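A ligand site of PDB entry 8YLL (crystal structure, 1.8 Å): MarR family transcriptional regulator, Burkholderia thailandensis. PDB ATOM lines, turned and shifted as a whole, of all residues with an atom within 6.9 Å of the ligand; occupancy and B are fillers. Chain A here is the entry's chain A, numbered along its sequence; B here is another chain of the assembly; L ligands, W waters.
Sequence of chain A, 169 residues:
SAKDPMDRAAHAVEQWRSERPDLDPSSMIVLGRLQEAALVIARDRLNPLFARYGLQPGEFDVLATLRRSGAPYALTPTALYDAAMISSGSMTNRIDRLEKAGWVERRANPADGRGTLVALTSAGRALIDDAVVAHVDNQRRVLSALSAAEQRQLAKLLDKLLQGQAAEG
NE1 of Trp 16 of chain B sits at hydrogen-bond distance from O1 of the ligand.
An oxygen (O1) of the ligand is in hydrogen-bond range of the guanidinium group of Arg 68.
The side-chain sulfur (SD) of Met 28 of chain B is in hydrogen-bond range of a nitrogen (N3) of the ligand, 3.4 Å away.
O2 of the ligand is in hydrogen-bond range of NE2 of His 135 (2.8 Å).
A nitrogen (N1) of the ligand is in hydrogen-bond range of the side-chain carboxylate (OD1) of Asp 61 (2.9 Å).
The backbone NH (N) of Ile 86 is in hydrogen-bond range of the side-chain carboxylate (OD2) of Asp 61 (3.3 Å).
NE2 of His 135 is in hydrogen-bond range of OE1 of Gln 139 (3.2 Å).
NH2 of Arg 68 is in hydrogen-bond range of OG1 of Thr 65, at 3.2 Å.
N of Met 28 of chain B sits close to NE2 of Gln 139, at 3.4 Å.
The guanidinium group (NH1) of Arg 68 lies within hydrogen-bond range of the backbone carbonyl oxygen (O) of Ala 83, 3.0 Å away.
NE2 of Gln 139 is in hydrogen-bond range of OG of Ser 27 of chain B, 2.8 Å away.
The side-chain hydroxyl of Thr 65 is in hydrogen-bond range of the backbone carbonyl oxygen of Asp 61 (2.8 Å).
The indole nitrogen (NE1) of Trp 16 of chain B lies close to the side-chain sulfur (SD) of Met 28 of chain B, 3.8 Å away.
Merely in contact with the ligand: Met 85, Gln 139, Ala 64 and Phe 60.
Within 4 Å of the ligand: Phe 60, Asp 61, Ala 64, Arg 68, Met 85, His 135, Gln 139, Trp 16 of chain B and Met 28 of chain B.
The nearest printed residue that does not touch the ligand is Ala 12 of chain B (4.2 Å).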
ATOM      1  N   LEU A  46     -26.694 -24.939   3.314  1.00  0.00           N
ATOM      2  CA  LEU A  46     -25.523 -24.087   3.310  1.00  0.00           C
ATOM      3  C   LEU A  46     -24.660 -24.313   4.541  1.00  0.00           C
ATOM      4  O   LEU A  46     -23.430 -24.444   4.437  1.00  0.00           O
ATOM      5  CB  LEU A  46     -25.938 -22.595   3.250  1.00  0.00           C
ATOM      6  CG  LEU A  46     -26.886 -22.185   2.113  1.00  0.00           C
ATOM      7  CD1 LEU A  46     -27.167 -20.685   2.175  1.00  0.00           C
ATOM      8  CD2 LEU A  46     -26.294 -22.565   0.759  1.00  0.00           C
ATOM      9  N   PHE A  50     -20.548 -25.156   5.208  1.00  0.00           N
ATOM     10  CA  PHE A  50     -19.632 -24.326   5.981  1.00  0.00           C
ATOM     11  C   PHE A  50     -18.978 -25.126   7.098  1.00  0.00           C
ATOM     12  O   PHE A  50     -17.787 -24.934   7.395  1.00  0.00           O
ATOM     13  CB  PHE A  50     -20.371 -23.121   6.550  1.00  0.00           C
ATOM     14  CG  PHE A  50     -20.977 -22.211   5.511  1.00  0.00           C
ATOM     15  CD1 PHE A  50     -20.350 -22.029   4.288  1.00  0.00           C
ATOM     16  CD2 PHE A  50     -22.150 -21.508   5.782  1.00  0.00           C
ATOM     17  CE1 PHE A  50     -20.901 -21.185   3.320  1.00  0.00           C
ATOM     18  CE2 PHE A  50     -22.712 -20.673   4.828  1.00  0.00           C
ATOM     19  CZ  PHE A  50     -22.081 -20.500   3.603  1.00  0.00           C
ATOM     20  N   GLY A  58     -22.288 -17.596   9.837  1.00  0.00           N
ATOM     21  CA  GLY A  58     -21.866 -16.225   9.972  1.00  0.00           C
ATOM     22  C   GLY A  58     -20.392 -16.010   9.781  1.00  0.00           C
ATOM     23  O   GLY A  58     -19.975 -14.914   9.371  1.00  0.00           O
ATOM     24  N   PHE A  60     -18.298 -17.751   7.665  1.00  0.00           N
ATOM     25  CA  PHE A  60     -18.051 -17.711   6.231  1.00  0.00           C
ATOM     26  C   PHE A  60     -18.228 -16.285   5.692  1.00  0.00           C
ATOM     27  O   PHE A  60     -17.370 -15.783   4.960  1.00  0.00           O
ATOM     28  CB  PHE A  60     -18.981 -18.662   5.496  1.00  0.00           C
ATOM     29  CG  PHE A  60     -18.822 -18.639   3.998  1.00  0.00           C
ATOM     30  CD1 PHE A  60     -17.911 -19.490   3.364  1.00  0.00           C
ATOM     31  CD2 PHE A  60     -19.589 -17.793   3.234  1.00  0.00           C
ATOM     32  CE1 PHE A  60     -17.762 -19.451   1.981  1.00  0.00           C
ATOM     33  CE2 PHE A  60     -19.449 -17.750   1.861  1.00  0.00           C
ATOM     34  CZ  PHE A  60     -18.534 -18.609   1.224  1.00  0.00           C
ATOM     35  N   ASP A  61     -19.348 -15.639   6.037  1.00  0.00           N
ATOM     36  CA  ASP A  61     -19.599 -14.285   5.551  1.00  0.00           C
ATOM     37  C   ASP A  61     -18.451 -13.345   5.895  1.00  0.00           C
ATOM     38  O   ASP A  61     -18.035 -12.537   5.063  1.00  0.00           O
ATOM     39  CB  ASP A  61     -20.931 -13.751   6.115  1.00  0.00           C
ATOM     40  CG  ASP A  61     -21.441 -12.504   5.364  1.00  0.00           C
ATOM     41  OD1 ASP A  61     -20.851 -12.151   4.306  1.00  0.00           O
ATOM     42  OD2 ASP A  61     -22.436 -11.870   5.812  1.00  0.00           O
ATOM     43  N   VAL A  62     -17.915 -13.428   7.124  1.00  0.00           N
ATOM     44  CA  VAL A  62     -16.809 -12.546   7.483  1.00  0.00           C
ATOM     45  C   VAL A  62     -15.625 -12.770   6.554  1.00  0.00           C
ATOM     46  O   VAL A  62     -15.096 -11.826   5.951  1.00  0.00           O
ATOM     47  CB  VAL A  62     -16.404 -12.727   8.959  1.00  0.00           C
ATOM     48  CG1 VAL A  62     -15.142 -11.895   9.223  1.00  0.00           C
ATOM     49  CG2 VAL A  62     -17.520 -12.307   9.896  1.00  0.00           C
ATOM     50  N   ALA A  64     -15.575 -14.208   3.666  1.00  0.00           N
ATOM     51  CA  ALA A  64     -15.919 -13.893   2.280  1.00  0.00           C
ATOM     52  C   ALA A  64     -15.855 -12.386   2.032  1.00  0.00           C
ATOM     53  O   ALA A  64     -15.330 -11.934   1.001  1.00  0.00           O
ATOM     54  CB  ALA A  64     -17.325 -14.422   1.972  1.00  0.00           C
ATOM     55  N   THR A  65     -16.357 -11.604   2.977  1.00  0.00           N
ATOM     56  CA  THR A  65     -16.307 -10.140   2.846  1.00  0.00           C
ATOM     57  C   THR A  65     -14.858  -9.644   2.771  1.00  0.00           C
ATOM     58  O   THR A  65     -14.504  -8.859   1.892  1.00  0.00           O
ATOM     59  CB  THR A  65     -17.061  -9.484   3.998  1.00  0.00           C
ATOM     60  OG1 THR A  65     -18.408  -9.986   4.048  1.00  0.00           O
ATOM     61  CG2 THR A  65     -17.112  -7.971   3.821  1.00  0.00           C
ATOM     62  N   ARG A  68     -13.213 -10.774  -0.664  1.00  0.00           N
ATOM     63  CA  ARG A  68     -13.616 -10.102  -1.896  1.00  0.00           C
ATOM     64  C   ARG A  68     -13.357  -8.600  -1.858  1.00  0.00           C
ATOM     65  O   ARG A  68     -13.565  -7.944  -2.881  1.00  0.00           O
ATOM     66  CB  ARG A  68     -15.090 -10.373  -2.219  1.00  0.00           C
ATOM     67  CG  ARG A  68     -16.070  -9.772  -1.274  1.00  0.00           C
ATOM     68  CD  ARG A  68     -17.457 -10.183  -1.718  1.00  0.00           C
ATOM     69  NE  ARG A  68     -18.322 -10.485  -0.583  1.00  0.00           N
ATOM     70  CZ  ARG A  68     -18.999  -9.563   0.107  1.00  0.00           C
ATOM     71  NH1 ARG A  68     -18.912  -8.272  -0.219  1.00  0.00           N
ATOM     72  NH2 ARG A  68     -19.755  -9.950   1.116  1.00  0.00           N
ATOM     73  N   ALA A  83     -20.292  -4.163   4.112  1.00  0.00           N
ATOM     74  CA  ALA A  83     -20.053  -4.971   2.923  1.00  0.00           C
ATOM     75  C   ALA A  83     -20.516  -6.411   3.064  1.00  0.00           C
ATOM     76  O   ALA A  83     -20.398  -7.183   2.101  1.00  0.00           O
ATOM     77  CB  ALA A  83     -18.570  -4.935   2.554  1.00  0.00           C
ATOM     78  N   ALA A  84     -21.036  -6.791   4.230  1.00  0.00           N
ATOM     79  CA  ALA A  84     -21.478  -8.165   4.443  1.00  0.00           C
ATOM     80  C   ALA A  84     -22.621  -8.518   3.490  1.00  0.00           C
ATOM     81  O   ALA A  84     -23.410  -7.669   3.090  1.00  0.00           O
ATOM     82  CB  ALA A  84     -21.936  -8.355   5.888  1.00  0.00           C
ATOM     83  N   MET A  85     -22.693  -9.797   3.102  1.00  0.00           N
ATOM     84  CA  MET A  85     -23.837 -10.249   2.323  1.00  0.00           C
ATOM     85  C   MET A  85     -25.139 -10.160   3.121  1.00  0.00           C
ATOM     86  O   MET A  85     -26.199  -9.853   2.565  1.00  0.00           O
ATOM     87  CB  MET A  85     -23.618 -11.703   1.878  1.00  0.00           C
ATOM     88  CG  MET A  85     -24.791 -12.311   1.161  1.00  0.00           C
ATOM     89  SD  MET A  85     -24.994 -11.666  -0.512  1.00  0.00           S
ATOM     90  CE  MET A  85     -23.583 -12.393  -1.364  1.00  0.00           C
ATOM     91  N   ILE A  86     -25.070 -10.421   4.430  1.00  0.00           N
ATOM     92  CA  ILE A  86     -26.223 -10.519   5.306  1.00  0.00           C
ATOM     93  C   ILE A  86     -25.982  -9.623   6.509  1.00  0.00           C
ATOM     94  O   ILE A  86     -24.904  -9.666   7.119  1.00  0.00           O
ATOM     95  CB  ILE A  86     -26.464 -11.973   5.763  1.00  0.00           C
ATOM     96  CG1 ILE A  86     -26.750 -12.874   4.551  1.00  0.00           C
ATOM     97  CG2 ILE A  86     -27.603 -12.036   6.771  1.00  0.00           C
ATOM     98  CD1 ILE A  86     -27.920 -12.401   3.707  1.00  0.00           C
ATOM     99  N   VAL A 132     -15.169 -20.957  -0.972  1.00  0.00           N
ATOM    100  CA  VAL A 132     -16.120 -20.229  -1.825  1.00  0.00           C
ATOM    101  C   VAL A 132     -16.433 -21.037  -3.084  1.00  0.00           C
ATOM    102  O   VAL A 132     -17.551 -20.965  -3.621  1.00  0.00           O
ATOM    103  CB  VAL A 132     -15.589 -18.824  -2.162  1.00  0.00           C
ATOM    104  CG1 VAL A 132     -14.391 -18.884  -3.091  1.00  0.00           C
ATOM    105  CG2 VAL A 132     -16.701 -17.987  -2.787  1.00  0.00           C
ATOM    106  N   HIS A 135     -18.914 -23.538  -2.011  1.00  0.00           N
ATOM    107  CA  HIS A 135     -20.145 -22.819  -1.690  1.00  0.00           C
ATOM    108  C   HIS A 135     -20.976 -22.528  -2.940  1.00  0.00           C
ATOM    109  O   HIS A 135     -22.192 -22.754  -2.939  1.00  0.00           O
ATOM    110  CB  HIS A 135     -19.790 -21.514  -0.957  1.00  0.00           C
ATOM    111  CG  HIS A 135     -20.967 -20.644  -0.681  1.00  0.00           C
ATOM    112  ND1 HIS A 135     -22.046 -21.045   0.073  1.00  0.00           N
ATOM    113  CD2 HIS A 135     -21.208 -19.350  -1.029  1.00  0.00           C
ATOM    114  CE1 HIS A 135     -22.906 -20.053   0.175  1.00  0.00           C
ATOM    115  NE2 HIS A 135     -22.435 -19.021  -0.501  1.00  0.00           N
ATOM    116  N   VAL A 136     -20.337 -22.058  -4.014  1.00  0.00           N
ATOM    117  CA  VAL A 136     -21.145 -21.704  -5.179  1.00  0.00           C
ATOM    118  C   VAL A 136     -21.669 -22.956  -5.880  1.00  0.00           C
ATOM    119  O   VAL A 136     -22.795 -22.950  -6.396  1.00  0.00           O
ATOM    120  CB  VAL A 136     -20.365 -20.790  -6.145  1.00  0.00           C
ATOM    121  CG1 VAL A 136     -20.226 -19.393  -5.533  1.00  0.00           C
ATOM    122  CG2 VAL A 136     -19.022 -21.359  -6.469  1.00  0.00           C
ATOM    123  N   GLN A 139     -24.673 -23.810  -3.907  1.00  0.00           N
ATOM    124  CA  GLN A 139     -25.782 -22.908  -4.193  1.00  0.00           C
ATOM    125  C   GLN A 139     -26.457 -23.274  -5.517  1.00  0.00           C
ATOM    126  O   GLN A 139     -27.686 -23.186  -5.636  1.00  0.00           O
ATOM    127  CB  GLN A 139     -25.301 -21.461  -4.219  1.00  0.00           C
ATOM    128  CG  GLN A 139     -24.911 -20.906  -2.879  1.00  0.00           C
ATOM    129  CD  GLN A 139     -24.874 -19.397  -2.879  1.00  0.00           C
ATOM    130  OE1 GLN A 139     -25.255 -18.745  -1.896  1.00  0.00           O
ATOM    131  NE2 GLN A 139     -24.432 -18.819  -3.992  1.00  0.00           N
ATOM    132  N   ALA B  12     -21.696  -7.598  -3.656  1.00  0.00           N
ATOM    133  CA  ALA B  12     -20.793  -8.696  -3.356  1.00  0.00           C
ATOM    134  C   ALA B  12     -20.477  -9.509  -4.603  1.00  0.00           C
ATOM    135  O   ALA B  12     -19.324  -9.899  -4.818  1.00  0.00           O
ATOM    136  CB  ALA B  12     -21.390  -9.593  -2.267  1.00  0.00           C
ATOM    137  N   VAL B  13     -21.486  -9.769  -5.452  1.00  0.00           N
ATOM    138  CA  VAL B  13     -21.239 -10.512  -6.694  1.00  0.00           C
ATOM    139  C   VAL B  13     -20.271  -9.735  -7.575  1.00  0.00           C
ATOM    140  O   VAL B  13     -19.397 -10.328  -8.215  1.00  0.00           O
ATOM    141  CB  VAL B  13     -22.569 -10.803  -7.412  1.00  0.00           C
ATOM    142  CG1 VAL B  13     -22.315 -11.218  -8.862  1.00  0.00           C
ATOM    143  CG2 VAL B  13     -23.324 -11.904  -6.686  1.00  0.00           C
ATOM    144  N   TRP B  16     -16.826 -10.286  -6.329  1.00  0.00           N
ATOM    145  CA  TRP B  16     -16.358 -11.652  -6.601  1.00  0.00           C
ATOM    146  C   TRP B  16     -15.930 -11.812  -8.053  1.00  0.00           C
ATOM    147  O   TRP B  16     -14.856 -12.363  -8.331  1.00  0.00           O
ATOM    148  CB  TRP B  16     -17.441 -12.665  -6.252  1.00  0.00           C
ATOM    149  CG  TRP B  16     -17.427 -13.084  -4.803  1.00  0.00           C
ATOM    150  CD1 TRP B  16     -18.458 -12.984  -3.920  1.00  0.00           C
ATOM    151  CD2 TRP B  16     -16.331 -13.663  -4.083  1.00  0.00           C
ATOM    152  NE1 TRP B  16     -18.075 -13.473  -2.685  1.00  0.00           N
ATOM    153  CE2 TRP B  16     -16.776 -13.898  -2.769  1.00  0.00           C
ATOM    154  CE3 TRP B  16     -15.021 -14.021  -4.440  1.00  0.00           C
ATOM    155  CZ2 TRP B  16     -15.944 -14.466  -1.792  1.00  0.00           C
ATOM    156  CZ3 TRP B  16     -14.200 -14.581  -3.467  1.00  0.00           C
ATOM    157  CH2 TRP B  16     -14.663 -14.796  -2.167  1.00  0.00           C
ATOM    158  N   SER B  27     -25.335 -17.334  -8.510  1.00  0.00           N
ATOM    159  CA  SER B  27     -26.299 -17.866  -7.540  1.00  0.00           C
ATOM    160  C   SER B  27     -26.357 -17.056  -6.253  1.00  0.00           C
ATOM    161  O   SER B  27     -27.350 -17.130  -5.521  1.00  0.00           O
ATOM    162  CB  SER B  27     -25.957 -19.322  -7.218  1.00  0.00           C
ATOM    163  OG  SER B  27     -24.627 -19.440  -6.717  1.00  0.00           O
ATOM    164  N   MET B  28     -25.319 -16.258  -5.970  1.00  0.00           N
ATOM    165  CA  MET B  28     -25.268 -15.503  -4.720  1.00  0.00           C
ATOM    166  C   MET B  28     -26.334 -14.415  -4.629  1.00  0.00           C
ATOM    167  O   MET B  28     -26.706 -14.014  -3.517  1.00  0.00           O
ATOM    168  CB  MET B  28     -23.884 -14.870  -4.560  1.00  0.00           C
ATOM    169  CG  MET B  28     -22.772 -15.866  -4.260  1.00  0.00           C
ATOM    170  SD  MET B  28     -21.227 -14.955  -4.154  1.00  0.00           S
ATOM    171  CE  MET B  28     -20.086 -16.265  -3.751  1.00  0.00           C
ATOM    172  N   ILE B  29     -26.816 -13.901  -5.754  1.00  0.00           N
ATOM    173  CA  ILE B  29     -27.791 -12.811  -5.692  1.00  0.00           C
ATOM    174  C   ILE B  29     -29.115 -13.309  -5.144  1.00  0.00           C
ATOM    175  O   ILE B  29     -29.611 -12.796  -4.126  1.00  0.00           O
ATOM    176  CB  ILE B  29     -27.956 -12.149  -7.073  1.00  0.00           C
ATOM    177  CG1 ILE B  29     -26.715 -11.311  -7.371  1.00  0.00           C
ATOM    178  CG2 ILE B  29     -29.191 -11.267  -7.101  1.00  0.00           C
ATOM    179  CD1 ILE B  29     -26.744 -10.600  -8.687  1.00  0.00           C
ATOM    180  N   LEU B  31     -29.922 -16.072  -3.541  1.00  0.00           N
ATOM    181  CA  LEU B  31     -29.881 -16.649  -2.201  1.00  0.00           C
ATOM    182  C   LEU B  31     -29.505 -15.603  -1.152  1.00  0.00           C
ATOM    183  O   LEU B  31     -29.994 -15.653  -0.021  1.00  0.00           O
ATOM    184  CB  LEU B  31     -28.894 -17.825  -2.154  1.00  0.00           C
ATOM    185  CG  LEU B  31     -29.443 -19.075  -2.858  1.00  0.00           C
ATOM    186  CD1 LEU B  31     -28.399 -20.197  -2.902  1.00  0.00           C
ATOM    187  CD2 LEU B  31     -30.696 -19.578  -2.160  1.00  0.00           C
ATOM    188  N   GLY B  32     -28.614 -14.682  -1.508  1.00  0.00           N
ATOM    189  CA  GLY B  32     -28.305 -13.585  -0.605  1.00  0.00           C
ATOM    190  C   GLY B  32     -29.512 -12.701  -0.343  1.00  0.00           C
ATOM    191  O   GLY B  32     -29.780 -12.323   0.806  1.00  0.00           O
ATOM    192  N   GLN B  35     -32.093 -14.647   1.976  1.00  0.00           N
ATOM    193  CA  GLN B  35     -31.759 -14.672   3.397  1.00  0.00           C
ATOM    194  C   GLN B  35     -31.836 -13.278   4.013  1.00  0.00           C
ATOM    195  O   GLN B  35     -32.266 -13.127   5.161  1.00  0.00           O
ATOM    196  CB  GLN B  35     -30.365 -15.265   3.589  1.00  0.00           C
ATOM    197  CG  GLN B  35     -30.294 -16.748   3.181  1.00  0.00           C
ATOM    198  CD  GLN B  35     -28.882 -17.310   3.223  1.00  0.00           C
ATOM    199  OE1 GLN B  35     -28.358 -17.590   4.303  1.00  0.00           O
ATOM    200  NE2 GLN B  35     -28.264 -17.467   2.060  1.00  0.00           N
HETATM  201  N1  LIG L   1     -22.010 -14.556   3.276  1.00  0.00           N
HETATM  202  C1  LIG L   1     -21.638 -14.455   1.962  1.00  0.00           C
HETATM  203  N2  LIG L   1     -20.728 -13.675   1.319  1.00  0.00           N
HETATM  204  C2  LIG L   1     -20.553 -13.780  -0.036  1.00  0.00           C
HETATM  205  O1  LIG L   1     -19.740 -13.072  -0.616  1.00  0.00           O
HETATM  206  N3  LIG L   1     -21.324 -14.699  -0.728  1.00  0.00           N
HETATM  207  C3  LIG L   1     -22.280 -15.537  -0.143  1.00  0.00           C
HETATM  208  O2  LIG L   1     -22.928 -16.319  -0.851  1.00  0.00           O
HETATM  209  C4  LIG L   1     -22.417 -15.375   1.264  1.00  0.00           C
HETATM  210  N4  LIG L   1     -23.255 -16.025   2.170  1.00  0.00           N
HETATM  211  C5  LIG L   1     -22.959 -15.500   3.334  1.00  0.00           C
HETATM  212  O   HOH W   1     -25.518 -15.684  -1.407  1.00  0.00           O
